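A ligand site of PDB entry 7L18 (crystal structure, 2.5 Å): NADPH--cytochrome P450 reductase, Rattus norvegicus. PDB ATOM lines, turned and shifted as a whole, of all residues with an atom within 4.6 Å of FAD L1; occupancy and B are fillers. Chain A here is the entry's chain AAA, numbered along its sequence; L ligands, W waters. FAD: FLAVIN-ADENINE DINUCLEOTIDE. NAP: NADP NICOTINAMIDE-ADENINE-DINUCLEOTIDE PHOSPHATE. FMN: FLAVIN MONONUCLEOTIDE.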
ATOM      1  N   TYR A  84       2.361  11.064 -23.152  1.00  0.00           N
ATOM      2  CA  TYR A  84       1.246  10.936 -22.177  1.00  0.00           C
ATOM      3  C   TYR A  84       1.861  10.549 -20.829  1.00  0.00           C
ATOM      4  O   TYR A  84       3.063  10.176 -20.813  1.00  0.00           O
ATOM      5  CB  TYR A  84       0.208   9.943 -22.700  1.00  0.00           C
ATOM      6  CG  TYR A  84      -1.132   9.962 -22.010  1.00  0.00           C
ATOM      7  CD1 TYR A  84      -1.960  11.079 -22.048  1.00  0.00           C
ATOM      8  CD2 TYR A  84      -1.597   8.858 -21.306  1.00  0.00           C
ATOM      9  CE1 TYR A  84      -3.188  11.098 -21.409  1.00  0.00           C
ATOM     10  CE2 TYR A  84      -2.816   8.866 -20.654  1.00  0.00           C
ATOM     11  CZ  TYR A  84      -3.618   9.988 -20.707  1.00  0.00           C
ATOM     12  OH  TYR A  84      -4.828   9.989 -20.082  1.00  0.00           O
ATOM     13  N   HIS A 263      -8.287   5.470 -13.556  1.00  0.00           N
ATOM     14  CA  HIS A 263      -9.081   6.428 -14.378  1.00  0.00           C
ATOM     15  C   HIS A 263     -10.355   5.746 -14.877  1.00  0.00           C
ATOM     16  O   HIS A 263     -10.302   4.553 -15.208  1.00  0.00           O
ATOM     17  CB  HIS A 263      -8.273   6.919 -15.583  1.00  0.00           C
ATOM     18  CG  HIS A 263      -6.965   7.571 -15.260  1.00  0.00           C
ATOM     19  ND1 HIS A 263      -6.743   8.256 -14.083  1.00  0.00           N
ATOM     20  CD2 HIS A 263      -5.846   7.711 -15.996  1.00  0.00           C
ATOM     21  CE1 HIS A 263      -5.530   8.756 -14.089  1.00  0.00           C
ATOM     22  NE2 HIS A 263      -4.961   8.439 -15.259  1.00  0.00           N
ATOM     23  N   THR A 322     -17.478  20.367 -31.451  1.00  0.00           N
ATOM     24  CA  THR A 322     -17.323  21.429 -30.424  1.00  0.00           C
ATOM     25  C   THR A 322     -15.919  22.045 -30.420  1.00  0.00           C
ATOM     26  O   THR A 322     -15.809  23.208 -29.976  1.00  0.00           O
ATOM     27  CB  THR A 322     -17.674  20.898 -29.042  1.00  0.00           C
ATOM     28  OG1 THR A 322     -16.868  19.758 -28.762  1.00  0.00           O
ATOM     29  CG2 THR A 322     -19.141  20.548 -28.960  1.00  0.00           C
ATOM     30  N   ARG A 368     -12.612  30.189 -29.980  1.00  0.00           N
ATOM     31  CA  ARG A 368     -13.204  28.854 -29.729  1.00  0.00           C
ATOM     32  C   ARG A 368     -14.450  28.683 -30.617  1.00  0.00           C
ATOM     33  O   ARG A 368     -15.508  28.264 -30.101  1.00  0.00           O
ATOM     34  CB  ARG A 368     -13.540  28.701 -28.248  1.00  0.00           C
ATOM     35  CG  ARG A 368     -12.644  27.718 -27.524  1.00  0.00           C
ATOM     36  CD  ARG A 368     -11.236  28.241 -27.361  1.00  0.00           C
ATOM     37  NE  ARG A 368     -10.642  27.823 -26.102  1.00  0.00           N
ATOM     38  CZ  ARG A 368      -9.346  27.942 -25.805  1.00  0.00           C
ATOM     39  NH1 ARG A 368      -8.500  28.441 -26.691  1.00  0.00           N
ATOM     40  NH2 ARG A 368      -8.913  27.529 -24.624  1.00  0.00           N
ATOM     41  N   ARG A 398     -13.715  10.840 -22.490  1.00  0.00           N
ATOM     42  CA  ARG A 398     -13.201  11.766 -21.452  1.00  0.00           C
ATOM     43  C   ARG A 398     -12.788  10.906 -20.259  1.00  0.00           C
ATOM     44  O   ARG A 398     -13.564  10.014 -19.886  1.00  0.00           O
ATOM     45  CB  ARG A 398     -14.251  12.829 -21.097  1.00  0.00           C
ATOM     46  CG  ARG A 398     -14.181  14.099 -21.927  1.00  0.00           C
ATOM     47  CD  ARG A 398     -14.503  13.894 -23.380  1.00  0.00           C
ATOM     48  NE  ARG A 398     -14.778  15.143 -24.065  1.00  0.00           N
ATOM     49  CZ  ARG A 398     -14.895  15.295 -25.378  1.00  0.00           C
ATOM     50  NH1 ARG A 398     -15.134  16.487 -25.895  1.00  0.00           N
ATOM     51  NH2 ARG A 398     -14.794  14.257 -26.190  1.00  0.00           N
ATOM     52  N   TYR A 399     -11.591  11.145 -19.703  1.00  0.00           N
ATOM     53  CA  TYR A 399     -11.067  10.455 -18.499  1.00  0.00           C
ATOM     54  C   TYR A 399     -11.400  11.257 -17.252  1.00  0.00           C
ATOM     55  O   TYR A 399     -11.469  12.501 -17.324  1.00  0.00           O
ATOM     56  CB  TYR A 399      -9.567  10.224 -18.608  1.00  0.00           C
ATOM     57  CG  TYR A 399      -9.157   9.350 -19.764  1.00  0.00           C
ATOM     58  CD1 TYR A 399      -9.240   7.969 -19.701  1.00  0.00           C
ATOM     59  CD2 TYR A 399      -8.686   9.917 -20.940  1.00  0.00           C
ATOM     60  CE1 TYR A 399      -8.864   7.163 -20.769  1.00  0.00           C
ATOM     61  CE2 TYR A 399      -8.304   9.127 -22.013  1.00  0.00           C
ATOM     62  CZ  TYR A 399      -8.403   7.751 -21.935  1.00  0.00           C
ATOM     63  OH  TYR A 399      -8.028   6.988 -23.010  1.00  0.00           O
ATOM     64  N   TYR A 400     -11.623  10.547 -16.142  1.00  0.00           N
ATOM     65  CA  TYR A 400     -11.849  11.088 -14.778  1.00  0.00           C
ATOM     66  C   TYR A 400     -11.128  10.209 -13.769  1.00  0.00           C
ATOM     67  O   TYR A 400     -11.189   8.983 -13.921  1.00  0.00           O
ATOM     68  CB  TYR A 400     -13.345  11.191 -14.480  1.00  0.00           C
ATOM     69  CG  TYR A 400     -14.062  12.072 -15.460  1.00  0.00           C
ATOM     70  CD1 TYR A 400     -14.591  11.550 -16.630  1.00  0.00           C
ATOM     71  CD2 TYR A 400     -14.145  13.435 -15.246  1.00  0.00           C
ATOM     72  CE1 TYR A 400     -15.212  12.375 -17.562  1.00  0.00           C
ATOM     73  CE2 TYR A 400     -14.770  14.274 -16.162  1.00  0.00           C
ATOM     74  CZ  TYR A 400     -15.292  13.732 -17.324  1.00  0.00           C
ATOM     75  OH  TYR A 400     -15.877  14.559 -18.235  1.00  0.00           O
ATOM     76  N   SER A 401     -10.429  10.811 -12.807  1.00  0.00           N
ATOM     77  CA  SER A 401      -9.814  10.103 -11.657  1.00  0.00           C
ATOM     78  C   SER A 401     -10.963   9.472 -10.880  1.00  0.00           C
ATOM     79  O   SER A 401     -11.897  10.222 -10.493  1.00  0.00           O
ATOM     80  CB  SER A 401      -9.026  11.034 -10.773  1.00  0.00           C
ATOM     81  OG  SER A 401      -7.858  11.515 -11.423  1.00  0.00           O
ATOM     82  N   CYS A 416     -15.781  12.730  -9.711  1.00  0.00           N
ATOM     83  CA  CYS A 416     -15.792  14.130  -9.210  1.00  0.00           C
ATOM     84  C   CYS A 416     -15.440  15.071 -10.361  1.00  0.00           C
ATOM     85  O   CYS A 416     -14.325  14.960 -10.860  1.00  0.00           O
ATOM     86  CB  CYS A 416     -14.778  14.274  -8.080  1.00  0.00           C
ATOM     87  SG  CYS A 416     -14.647  15.965  -7.452  1.00  0.00           S
ATOM     88  N   ALA A 417     -16.351  15.918 -10.828  1.00  0.00           N
ATOM     89  CA  ALA A 417     -16.117  16.742 -12.043  1.00  0.00           C
ATOM     90  C   ALA A 417     -16.654  18.159 -11.872  1.00  0.00           C
ATOM     91  O   ALA A 417     -17.746  18.279 -11.306  1.00  0.00           O
ATOM     92  CB  ALA A 417     -16.768  16.083 -13.230  1.00  0.00           C
ATOM     93  N   VAL A 418     -15.944  19.160 -12.406  1.00  0.00           N
ATOM     94  CA  VAL A 418     -16.479  20.528 -12.681  1.00  0.00           C
ATOM     95  C   VAL A 418     -17.118  20.500 -14.077  1.00  0.00           C
ATOM     96  O   VAL A 418     -16.462  20.068 -15.032  1.00  0.00           O
ATOM     97  CB  VAL A 418     -15.427  21.659 -12.520  1.00  0.00           C
ATOM     98  CG1 VAL A 418     -14.118  21.407 -13.244  1.00  0.00           C
ATOM     99  CG2 VAL A 418     -15.993  23.014 -12.939  1.00  0.00           C
ATOM    100  N   VAL A 420     -18.158  22.120 -17.458  1.00  0.00           N
ATOM    101  CA  VAL A 420     -17.498  23.174 -18.290  1.00  0.00           C
ATOM    102  C   VAL A 420     -18.587  23.939 -19.021  1.00  0.00           C
ATOM    103  O   VAL A 420     -19.382  23.298 -19.731  1.00  0.00           O
ATOM    104  CB  VAL A 420     -16.455  22.611 -19.266  1.00  0.00           C
ATOM    105  CG1 VAL A 420     -15.981  23.683 -20.236  1.00  0.00           C
ATOM    106  CG2 VAL A 420     -15.263  22.007 -18.543  1.00  0.00           C
ATOM    107  N   TYR A 422     -18.627  28.110 -20.460  1.00  0.00           N
ATOM    108  CA  TYR A 422     -17.888  29.387 -20.473  1.00  0.00           C
ATOM    109  C   TYR A 422     -18.355  30.229 -21.643  1.00  0.00           C
ATOM    110  O   TYR A 422     -18.906  29.675 -22.594  1.00  0.00           O
ATOM    111  CB  TYR A 422     -16.373  29.154 -20.533  1.00  0.00           C
ATOM    112  CG  TYR A 422     -15.888  28.459 -21.782  1.00  0.00           C
ATOM    113  CD1 TYR A 422     -15.800  27.084 -21.827  1.00  0.00           C
ATOM    114  CD2 TYR A 422     -15.470  29.170 -22.897  1.00  0.00           C
ATOM    115  CE1 TYR A 422     -15.328  26.420 -22.944  1.00  0.00           C
ATOM    116  CE2 TYR A 422     -14.985  28.524 -24.025  1.00  0.00           C
ATOM    117  CZ  TYR A 422     -14.922  27.144 -24.056  1.00  0.00           C
ATOM    118  OH  TYR A 422     -14.471  26.456 -25.134  1.00  0.00           O
ATOM    119  N   LYS A 431     -20.149  24.693 -24.117  1.00  0.00           N
ATOM    120  CA  LYS A 431     -20.459  23.669 -23.087  1.00  0.00           C
ATOM    121  C   LYS A 431     -19.507  22.488 -23.307  1.00  0.00           C
ATOM    122  O   LYS A 431     -19.285  22.116 -24.454  1.00  0.00           O
ATOM    123  CB  LYS A 431     -21.942  23.322 -23.175  1.00  0.00           C
ATOM    124  CG  LYS A 431     -22.852  24.542 -23.074  1.00  0.00           C
ATOM    125  CD  LYS A 431     -24.205  24.263 -22.473  1.00  0.00           C
ATOM    126  CE  LYS A 431     -24.142  24.005 -20.984  1.00  0.00           C
ATOM    127  NZ  LYS A 431     -25.022  22.864 -20.636  1.00  0.00           N
ATOM    128  N   GLY A 432     -18.902  22.007 -22.237  1.00  0.00           N
ATOM    129  CA  GLY A 432     -18.159  20.733 -22.200  1.00  0.00           C
ATOM    130  C   GLY A 432     -19.062  19.594 -22.617  1.00  0.00           C
ATOM    131  O   GLY A 432     -20.180  19.475 -22.078  1.00  0.00           O
ATOM    132  N   VAL A 433     -18.601  18.777 -23.558  1.00  0.00           N
ATOM    133  CA  VAL A 433     -19.439  17.690 -24.131  1.00  0.00           C
ATOM    134  C   VAL A 433     -19.792  16.703 -23.020  1.00  0.00           C
ATOM    135  O   VAL A 433     -20.982  16.474 -22.773  1.00  0.00           O
ATOM    136  CB  VAL A 433     -18.719  16.994 -25.294  1.00  0.00           C
ATOM    137  CG1 VAL A 433     -19.555  15.851 -25.843  1.00  0.00           C
ATOM    138  CG2 VAL A 433     -18.348  17.993 -26.392  1.00  0.00           C
ATOM    139  N   ALA A 434     -18.779  16.134 -22.395  1.00  0.00           N
ATOM    140  CA  ALA A 434     -18.962  15.042 -21.413  1.00  0.00           C
ATOM    141  C   ALA A 434     -19.598  15.582 -20.115  1.00  0.00           C
ATOM    142  O   ALA A 434     -20.517  14.919 -19.583  1.00  0.00           O
ATOM    143  CB  ALA A 434     -17.621  14.392 -21.166  1.00  0.00           C
ATOM    144  N   THR A 435     -19.150  16.730 -19.613  1.00  0.00           N
ATOM    145  CA  THR A 435     -19.638  17.310 -18.327  1.00  0.00           C
ATOM    146  C   THR A 435     -21.102  17.727 -18.462  1.00  0.00           C
ATOM    147  O   THR A 435     -21.860  17.460 -17.523  1.00  0.00           O
ATOM    148  CB  THR A 435     -18.764  18.473 -17.850  1.00  0.00           C
ATOM    149  OG1 THR A 435     -18.676  19.446 -18.899  1.00  0.00           O
ATOM    150  CG2 THR A 435     -17.392  18.028 -17.411  1.00  0.00           C
ATOM    151  N   THR A 479     -10.829  19.967  -7.913  1.00  0.00           N
ATOM    152  CA  THR A 479     -11.192  18.595  -8.342  1.00  0.00           C
ATOM    153  C   THR A 479      -9.939  17.714  -8.253  1.00  0.00           C
ATOM    154  O   THR A 479     -10.082  16.497  -8.444  1.00  0.00           O
ATOM    155  CB  THR A 479     -11.818  18.554  -9.759  1.00  0.00           C
ATOM    156  OG1 THR A 479     -10.882  18.998 -10.732  1.00  0.00           O
ATOM    157  CG2 THR A 479     -13.070  19.397  -9.883  1.00  0.00           C
ATOM    158  N   ALA A 482     -10.054  14.417  -6.464  1.00  0.00           N
ATOM    159  CA  ALA A 482     -10.848  13.277  -6.979  1.00  0.00           C
ATOM    160  C   ALA A 482     -10.253  11.955  -6.476  1.00  0.00           C
ATOM    161  O   ALA A 482     -10.923  11.234  -5.751  1.00  0.00           O
ATOM    162  CB  ALA A 482     -10.973  13.325  -8.489  1.00  0.00           C
ATOM    163  N   TRP A 619      -3.574  17.147 -15.174  1.00  0.00           N
ATOM    164  CA  TRP A 619      -4.323  17.428 -16.426  1.00  0.00           C
ATOM    165  C   TRP A 619      -4.579  18.939 -16.549  1.00  0.00           C
ATOM    166  O   TRP A 619      -4.554  19.631 -15.512  1.00  0.00           O
ATOM    167  CB  TRP A 619      -5.626  16.607 -16.489  1.00  0.00           C
ATOM    168  CG  TRP A 619      -6.730  17.109 -15.600  1.00  0.00           C
ATOM    169  CD1 TRP A 619      -7.611  18.101 -15.881  1.00  0.00           C
ATOM    170  CD2 TRP A 619      -7.058  16.623 -14.287  1.00  0.00           C
ATOM    171  NE1 TRP A 619      -8.477  18.280 -14.830  1.00  0.00           N
ATOM    172  CE2 TRP A 619      -8.158  17.397 -13.833  1.00  0.00           C
ATOM    173  CE3 TRP A 619      -6.556  15.622 -13.440  1.00  0.00           C
ATOM    174  CZ2 TRP A 619      -8.742  17.191 -12.584  1.00  0.00           C
ATOM    175  CZ3 TRP A 619      -7.138  15.416 -12.209  1.00  0.00           C
ATOM    176  CH2 TRP A 619      -8.223  16.199 -11.788  1.00  0.00           C
HETATM  177  PA  FAD L   1     -14.663  19.555 -23.694  1.00  0.00           P
HETATM  178  O1A FAD L   1     -15.918  19.765 -24.463  1.00  0.00           O
HETATM  179  O2A FAD L   1     -13.712  18.476 -24.066  1.00  0.00           O
HETATM  180  O5B FAD L   1     -13.882  20.933 -23.616  1.00  0.00           O
HETATM  181  C5B FAD L   1     -12.571  20.995 -23.043  1.00  0.00           C
HETATM  182  C4B FAD L   1     -11.938  22.270 -23.533  1.00  0.00           C
HETATM  183  O4B FAD L   1     -12.754  23.402 -23.151  1.00  0.00           O
HETATM  184  C3B FAD L   1     -10.567  22.622 -22.958  1.00  0.00           C
HETATM  185  O3B FAD L   1      -9.531  21.897 -23.613  1.00  0.00           O
HETATM  186  C2B FAD L   1     -10.498  24.110 -23.298  1.00  0.00           C
HETATM  187  O2B FAD L   1     -10.027  24.308 -24.607  1.00  0.00           O
HETATM  188  C1B FAD L   1     -11.952  24.567 -23.235  1.00  0.00           C
HETATM  189  N9A FAD L   1     -12.260  25.470 -22.114  1.00  0.00           N
HETATM  190  C8A FAD L   1     -12.697  25.176 -20.823  1.00  0.00           C
HETATM  191  N7A FAD L   1     -12.908  26.258 -20.107  1.00  0.00           N
HETATM  192  C5A FAD L   1     -12.596  27.313 -20.957  1.00  0.00           C
HETATM  193  C6A FAD L   1     -12.614  28.716 -20.800  1.00  0.00           C
HETATM  194  N6A FAD L   1     -13.005  29.325 -19.683  1.00  0.00           N
HETATM  195  N1A FAD L   1     -12.241  29.478 -21.852  1.00  0.00           N
HETATM  196  C2A FAD L   1     -11.867  28.858 -22.982  1.00  0.00           C
HETATM  197  N3A FAD L   1     -11.817  27.558 -23.253  1.00  0.00           N
HETATM  198  C4A FAD L   1     -12.202  26.837 -22.186  1.00  0.00           C
HETATM  199  N1  FAD L   1     -11.998  16.509 -14.992  1.00  0.00           N
HETATM  200  C2  FAD L   1     -12.635  16.621 -13.849  1.00  0.00           C
HETATM  201  O2  FAD L   1     -13.503  17.469 -13.700  1.00  0.00           O
HETATM  202  N3  FAD L   1     -12.388  15.767 -12.803  1.00  0.00           N
HETATM  203  C4  FAD L   1     -11.446  14.787 -12.864  1.00  0.00           C
HETATM  204  O4  FAD L   1     -11.274  14.035 -11.917  1.00  0.00           O
HETATM  205  C4X FAD L   1     -10.702  14.683 -14.065  1.00  0.00           C
HETATM  206  N5  FAD L   1      -9.742  13.793 -14.167  1.00  0.00           N
HETATM  207  C5X FAD L   1      -9.038  13.746 -15.333  1.00  0.00           C
HETATM  208  C6  FAD L   1      -8.000  12.807 -15.459  1.00  0.00           C
HETATM  209  C7  FAD L   1      -7.265  12.696 -16.614  1.00  0.00           C
HETATM  210  C7M FAD L   1      -6.180  11.652 -16.716  1.00  0.00           C
HETATM  211  C8  FAD L   1      -7.556  13.551 -17.718  1.00  0.00           C
HETATM  212  C8M FAD L   1      -6.774  13.466 -19.007  1.00  0.00           C
HETATM  213  C9  FAD L   1      -8.570  14.466 -17.600  1.00  0.00           C
HETATM  214  C9A FAD L   1      -9.320  14.590 -16.423  1.00  0.00           C
HETATM  215  N10 FAD L   1     -10.341  15.520 -16.271  1.00  0.00           N
HETATM  216  C10 FAD L   1     -11.062  15.613 -15.097  1.00  0.00           C
HETATM  217  C1' FAD L   1     -10.713  16.392 -17.408  1.00  0.00           C
HETATM  218  C2' FAD L   1     -11.690  15.643 -18.295  1.00  0.00           C
HETATM  219  O2' FAD L   1     -11.020  14.579 -19.015  1.00  0.00           O
HETATM  220  C3' FAD L   1     -12.435  16.554 -19.273  1.00  0.00           C
HETATM  221  O3' FAD L   1     -11.533  17.190 -20.155  1.00  0.00           O
HETATM  222  C4' FAD L   1     -13.276  17.664 -18.632  1.00  0.00           C
HETATM  223  O4' FAD L   1     -14.267  17.124 -17.750  1.00  0.00           O
HETATM  224  C5' FAD L   1     -13.965  18.482 -19.688  1.00  0.00           C
HETATM  225  O5' FAD L   1     -14.477  17.585 -20.732  1.00  0.00           O
HETATM  226  P   FAD L   1     -15.776  18.052 -21.529  1.00  0.00           P
HETATM  227  O1P FAD L   1     -16.881  18.396 -20.597  1.00  0.00           O
HETATM  228  O2P FAD L   1     -16.073  16.995 -22.538  1.00  0.00           O
HETATM  229  O3P FAD L   1     -15.137  19.350 -22.188  1.00  0.00           O
HETATM  230  PA  NAP L   2     -10.157  25.689  -9.251  1.00  0.00           P
HETATM  231  O1A NAP L   2     -11.303  25.538  -8.320  1.00  0.00           O
HETATM  232  O2A NAP L   2     -10.109  26.940 -10.066  1.00  0.00           O
HETATM  233  O5B NAP L   2      -8.812  25.532  -8.408  1.00  0.00           O
HETATM  234  C5B NAP L   2      -8.931  24.956  -7.085  1.00  0.00           C
HETATM  235  C4B NAP L   2      -8.189  25.809  -6.083  1.00  0.00           C
HETATM  236  O4B NAP L   2      -6.813  25.942  -6.510  1.00  0.00           O
HETATM  237  C3B NAP L   2      -8.718  27.231  -5.853  1.00  0.00           C
HETATM  238  O3B NAP L   2      -8.836  27.530  -4.466  1.00  0.00           O
HETATM  239  C2B NAP L   2      -7.665  28.091  -6.553  1.00  0.00           C
HETATM  240  O2B NAP L   2      -7.556  29.411  -6.013  1.00  0.00           O
HETATM  241  C1B NAP L   2      -6.427  27.254  -6.245  1.00  0.00           C
HETATM  242  N9A NAP L   2      -5.263  27.590  -7.038  1.00  0.00           N
HETATM  243  C8A NAP L   2      -5.245  28.347  -8.184  1.00  0.00           C
HETATM  244  N7A NAP L   2      -4.033  28.535  -8.654  1.00  0.00           N
HETATM  245  C5A NAP L   2      -3.207  27.907  -7.742  1.00  0.00           C
HETATM  246  C6A NAP L   2      -1.811  27.769  -7.690  1.00  0.00           C
HETATM  247  N6A NAP L   2      -0.983  28.300  -8.596  1.00  0.00           N
HETATM  248  N1A NAP L   2      -1.288  27.087  -6.632  1.00  0.00           N
HETATM  249  C2A NAP L   2      -2.141  26.572  -5.724  1.00  0.00           C
HETATM  250  N3A NAP L   2      -3.477  26.627  -5.697  1.00  0.00           N
HETATM  251  C4A NAP L   2      -3.947  27.314  -6.743  1.00  0.00           C
HETATM  252  O3  NAP L   2     -10.105  24.444 -10.244  1.00  0.00           O
HETATM  253  PN  NAP L   2     -11.178  23.259 -10.360  1.00  0.00           P
HETATM  254  O1N NAP L   2     -12.455  23.668  -9.688  1.00  0.00           O
HETATM  255  O2N NAP L   2     -10.545  22.018  -9.843  1.00  0.00           O
HETATM  256  O5D NAP L   2     -11.431  23.107 -11.940  1.00  0.00           O
HETATM  257  C5D NAP L   2     -11.036  24.041 -12.975  1.00  0.00           C
HETATM  258  C4D NAP L   2     -10.548  23.276 -14.182  1.00  0.00           C
HETATM  259  O4D NAP L   2     -10.906  23.996 -15.390  1.00  0.00           O
HETATM  260  C3D NAP L   2      -9.027  23.030 -14.259  1.00  0.00           C
HETATM  261  O3D NAP L   2      -8.678  21.762 -14.815  1.00  0.00           O
HETATM  262  C2D NAP L   2      -8.554  24.185 -15.138  1.00  0.00           C
HETATM  263  O2D NAP L   2      -7.339  23.871 -15.802  1.00  0.00           O
HETATM  264  C1D NAP L   2      -9.727  24.369 -16.100  1.00  0.00           C
HETATM  265  N1N NAP L   2      -9.864  25.781 -16.585  1.00  0.00           N
HETATM  266  C2N NAP L   2      -9.441  26.109 -17.850  1.00  0.00           C
HETATM  267  C3N NAP L   2      -9.446  27.438 -18.294  1.00  0.00           C
HETATM  268  C7N NAP L   2      -9.003  27.698 -19.712  1.00  0.00           C
HETATM  269  O7N NAP L   2      -8.824  26.760 -20.476  1.00  0.00           O
HETATM  270  N7N NAP L   2      -8.812  28.965 -20.080  1.00  0.00           N
HETATM  271  C4N NAP L   2      -9.876  28.434 -17.399  1.00  0.00           C
HETATM  272  C5N NAP L   2     -10.393  28.076 -16.169  1.00  0.00           C
HETATM  273  C6N NAP L   2     -10.401  26.756 -15.784  1.00  0.00           C
HETATM  274  P2B NAP L   2      -8.010  30.688  -6.923  1.00  0.00           P
HETATM  275  O1X NAP L   2      -6.641  31.211  -7.346  1.00  0.00           O
HETATM  276  O2X NAP L   2      -8.771  31.709  -6.067  1.00  0.00           O
HETATM  277  O3X NAP L   2      -8.836  30.265  -8.106  1.00  0.00           O
HETATM  278  N1  FMN L   3       3.143  16.284 -23.026  1.00  0.00           N
HETATM  279  C2  FMN L   3       4.464  16.169 -22.727  1.00  0.00           C
HETATM  280  O2  FMN L   3       5.312  16.728 -23.422  1.00  0.00           O
HETATM  281  N3  FMN L   3       4.902  15.401 -21.684  1.00  0.00           N
HETATM  282  C4  FMN L   3       4.029  14.711 -20.873  1.00  0.00           C
HETATM  283  O4  FMN L   3       4.477  14.050 -19.940  1.00  0.00           O
HETATM  284  C4A FMN L   3       2.644  14.858 -21.110  1.00  0.00           C
HETATM  285  N5  FMN L   3       1.798  14.245 -20.326  1.00  0.00           N
HETATM  286  C5A FMN L   3       0.466  14.448 -20.552  1.00  0.00           C
HETATM  287  C6  FMN L   3      -0.438  13.834 -19.664  1.00  0.00           C
HETATM  288  C7  FMN L   3      -1.792  14.007 -19.793  1.00  0.00           C
HETATM  289  C7M FMN L   3      -2.710  13.337 -18.808  1.00  0.00           C
HETATM  290  C8  FMN L   3      -2.308  14.799 -20.864  1.00  0.00           C
HETATM  291  C8M FMN L   3      -3.789  15.000 -21.044  1.00  0.00           C
HETATM  292  C9  FMN L   3      -1.424  15.372 -21.759  1.00  0.00           C
HETATM  293  C9A FMN L   3      -0.031  15.237 -21.608  1.00  0.00           C
HETATM  294  N10 FMN L   3       0.900  15.830 -22.475  1.00  0.00           N
HETATM  295  C10 FMN L   3       2.264  15.685 -22.234  1.00  0.00           C
HETATM  296  C1' FMN L   3       0.443  16.668 -23.609  1.00  0.00           C
HETATM  297  C2' FMN L   3       0.027  15.822 -24.817  1.00  0.00           C
HETATM  298  O2' FMN L   3       1.152  15.136 -25.380  1.00  0.00           O
HETATM  299  C3' FMN L   3      -0.624  16.646 -25.927  1.00  0.00           C
HETATM  300  O3' FMN L   3      -1.904  17.130 -25.524  1.00  0.00           O
HETATM  301  C4' FMN L   3      -0.783  15.868 -27.234  1.00  0.00           C
HETATM  302  O4' FMN L   3      -1.264  16.750 -28.250  1.00  0.00           O
HETATM  303  C5' FMN L   3      -1.747  14.705 -27.105  1.00  0.00           C
HETATM  304  O5' FMN L   3      -1.817  14.056 -28.392  1.00  0.00           O
HETATM  305  P   FMN L   3      -2.887  12.902 -28.636  1.00  0.00           P
HETATM  306  O1P FMN L   3      -4.236  13.546 -28.838  1.00  0.00           O
HETATM  307  O2P FMN L   3      -2.790  11.993 -27.421  1.00  0.00           O
HETATM  308  O3P FMN L   3      -2.422  12.231 -29.911  1.00  0.00           O
HETATM  309  O   HOH W   1      -9.713  31.356 -21.884  1.00  0.00           O
HETATM  310  O   HOH W   2     -12.191  17.994 -26.110  1.00  0.00           O
HETATM  311  O   HOH W   3      -3.461  12.613 -15.225  1.00  0.00           O
HETATM  312  O   HOH W   4     -10.143  13.143 -21.116  1.00  0.00           O
HETATM  313  O   HOH W   5     -13.416  12.158 -11.094  1.00  0.00           O
HETATM  314  O   HOH W   6     -14.114  18.805 -15.717  1.00  0.00           O
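Merely in contact with FAD L1: Gly 432, Ala 417, Trp 619, Ala 482, Val 420, His 263 and Tyr 84.
18 residues have an atom within 4 Å of FAD L1: Tyr 84, His 263, Arg 368, Arg 398, Tyr 399, Tyr 400, Ser 401, Cys 416, Ala 417, Val 418, Val 420, Tyr 422, Gly 432, Val 433, Ala 434, Thr 435, Ala 482 and Trp 619.
The nearest printed residue that does not touch FAD L1 is Lys 431 (4.1 Å).
O1A of FAD L1 sits at hydrogen-bond distance from N of Val 433, at 3.0 Å.
N of Val 418 lies within hydrogen-bond range of O2 of FAD L1.
An oxygen (O3D) of NAP L2 sits at hydrogen-bond distance from the indole nitrogen (NE1) of Trp 619 (3.5 Å).
O of Cys 416 is in hydrogen-bond range of N3 of FAD L1 (2.9 Å).
A nitrogen (N3A) of FAD L1 sits close to the side-chain hydroxyl (OH) of Tyr 422 (3.4 Å).
O2N of NAP L2 lies within hydrogen-bond range of N of Thr 479, at 2.8 Å.
OG1 of Thr 435 is in hydrogen-bond range of O1P of FAD L1, 2.7 Å away.
An oxygen (O2P) of FAD L1 lies within hydrogen-bond range of the backbone NH (N) of Ala 434, at 2.8 Å.
N of Thr 435 is in hydrogen-bond range of O1P of FAD L1, 3.0 Å away.
O4' of FAD L1 is in hydrogen-bond range of OH of Tyr 400 (3.1 Å).
The guanidinium group (NE) of Arg 398 lies within salt-bridge range of an oxygen (O2P) of FAD L1, at 2.7 Å.
An oxygen (O2N) of NAP L2 lies within hydrogen-bond range of the side-chain hydroxyl of Thr 479 (3.2 Å).
N of Ser 401 lies within hydrogen-bond range of N5 of FAD L1 (3.3 Å).
The guanidinium group (NE) of Arg 368 is in hydrogen-bond range of a nitrogen (N3A) of FAD L1.
O2' of FAD L1 sits at hydrogen-bond distance from O of Tyr 399.
The side-chain hydroxyl (OG1) of Thr 435 sits at hydrogen-bond distance from the backbone NH (N) of Val 420, 3.1 Å away.
N of Gly 432 lies within hydrogen-bond range of O of Val 420.
Water W6 bridges an oxygen (O2) of FAD L1 (2.5 Å) and the backbone carbonyl oxygen of Val 418 (2.8 Å).
Water W2 lies within hydrogen-bond range of O2A of FAD L1 (2.6 Å) and NH1 of Arg 398 (3.3 Å).
Water W4 bridges O2' of FAD L1 and N of Tyr 399.
Water W5 lies within hydrogen-bond range of O of Ser 401 (2.5 Å), N of Cys 416 (2.8 Å) and O4 of FAD L1 (3.0 Å).
Water W1 lies within hydrogen-bond range of N7N of NAP L2 (3.1 Å) and N1A of FAD L1 (3.1 Å).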
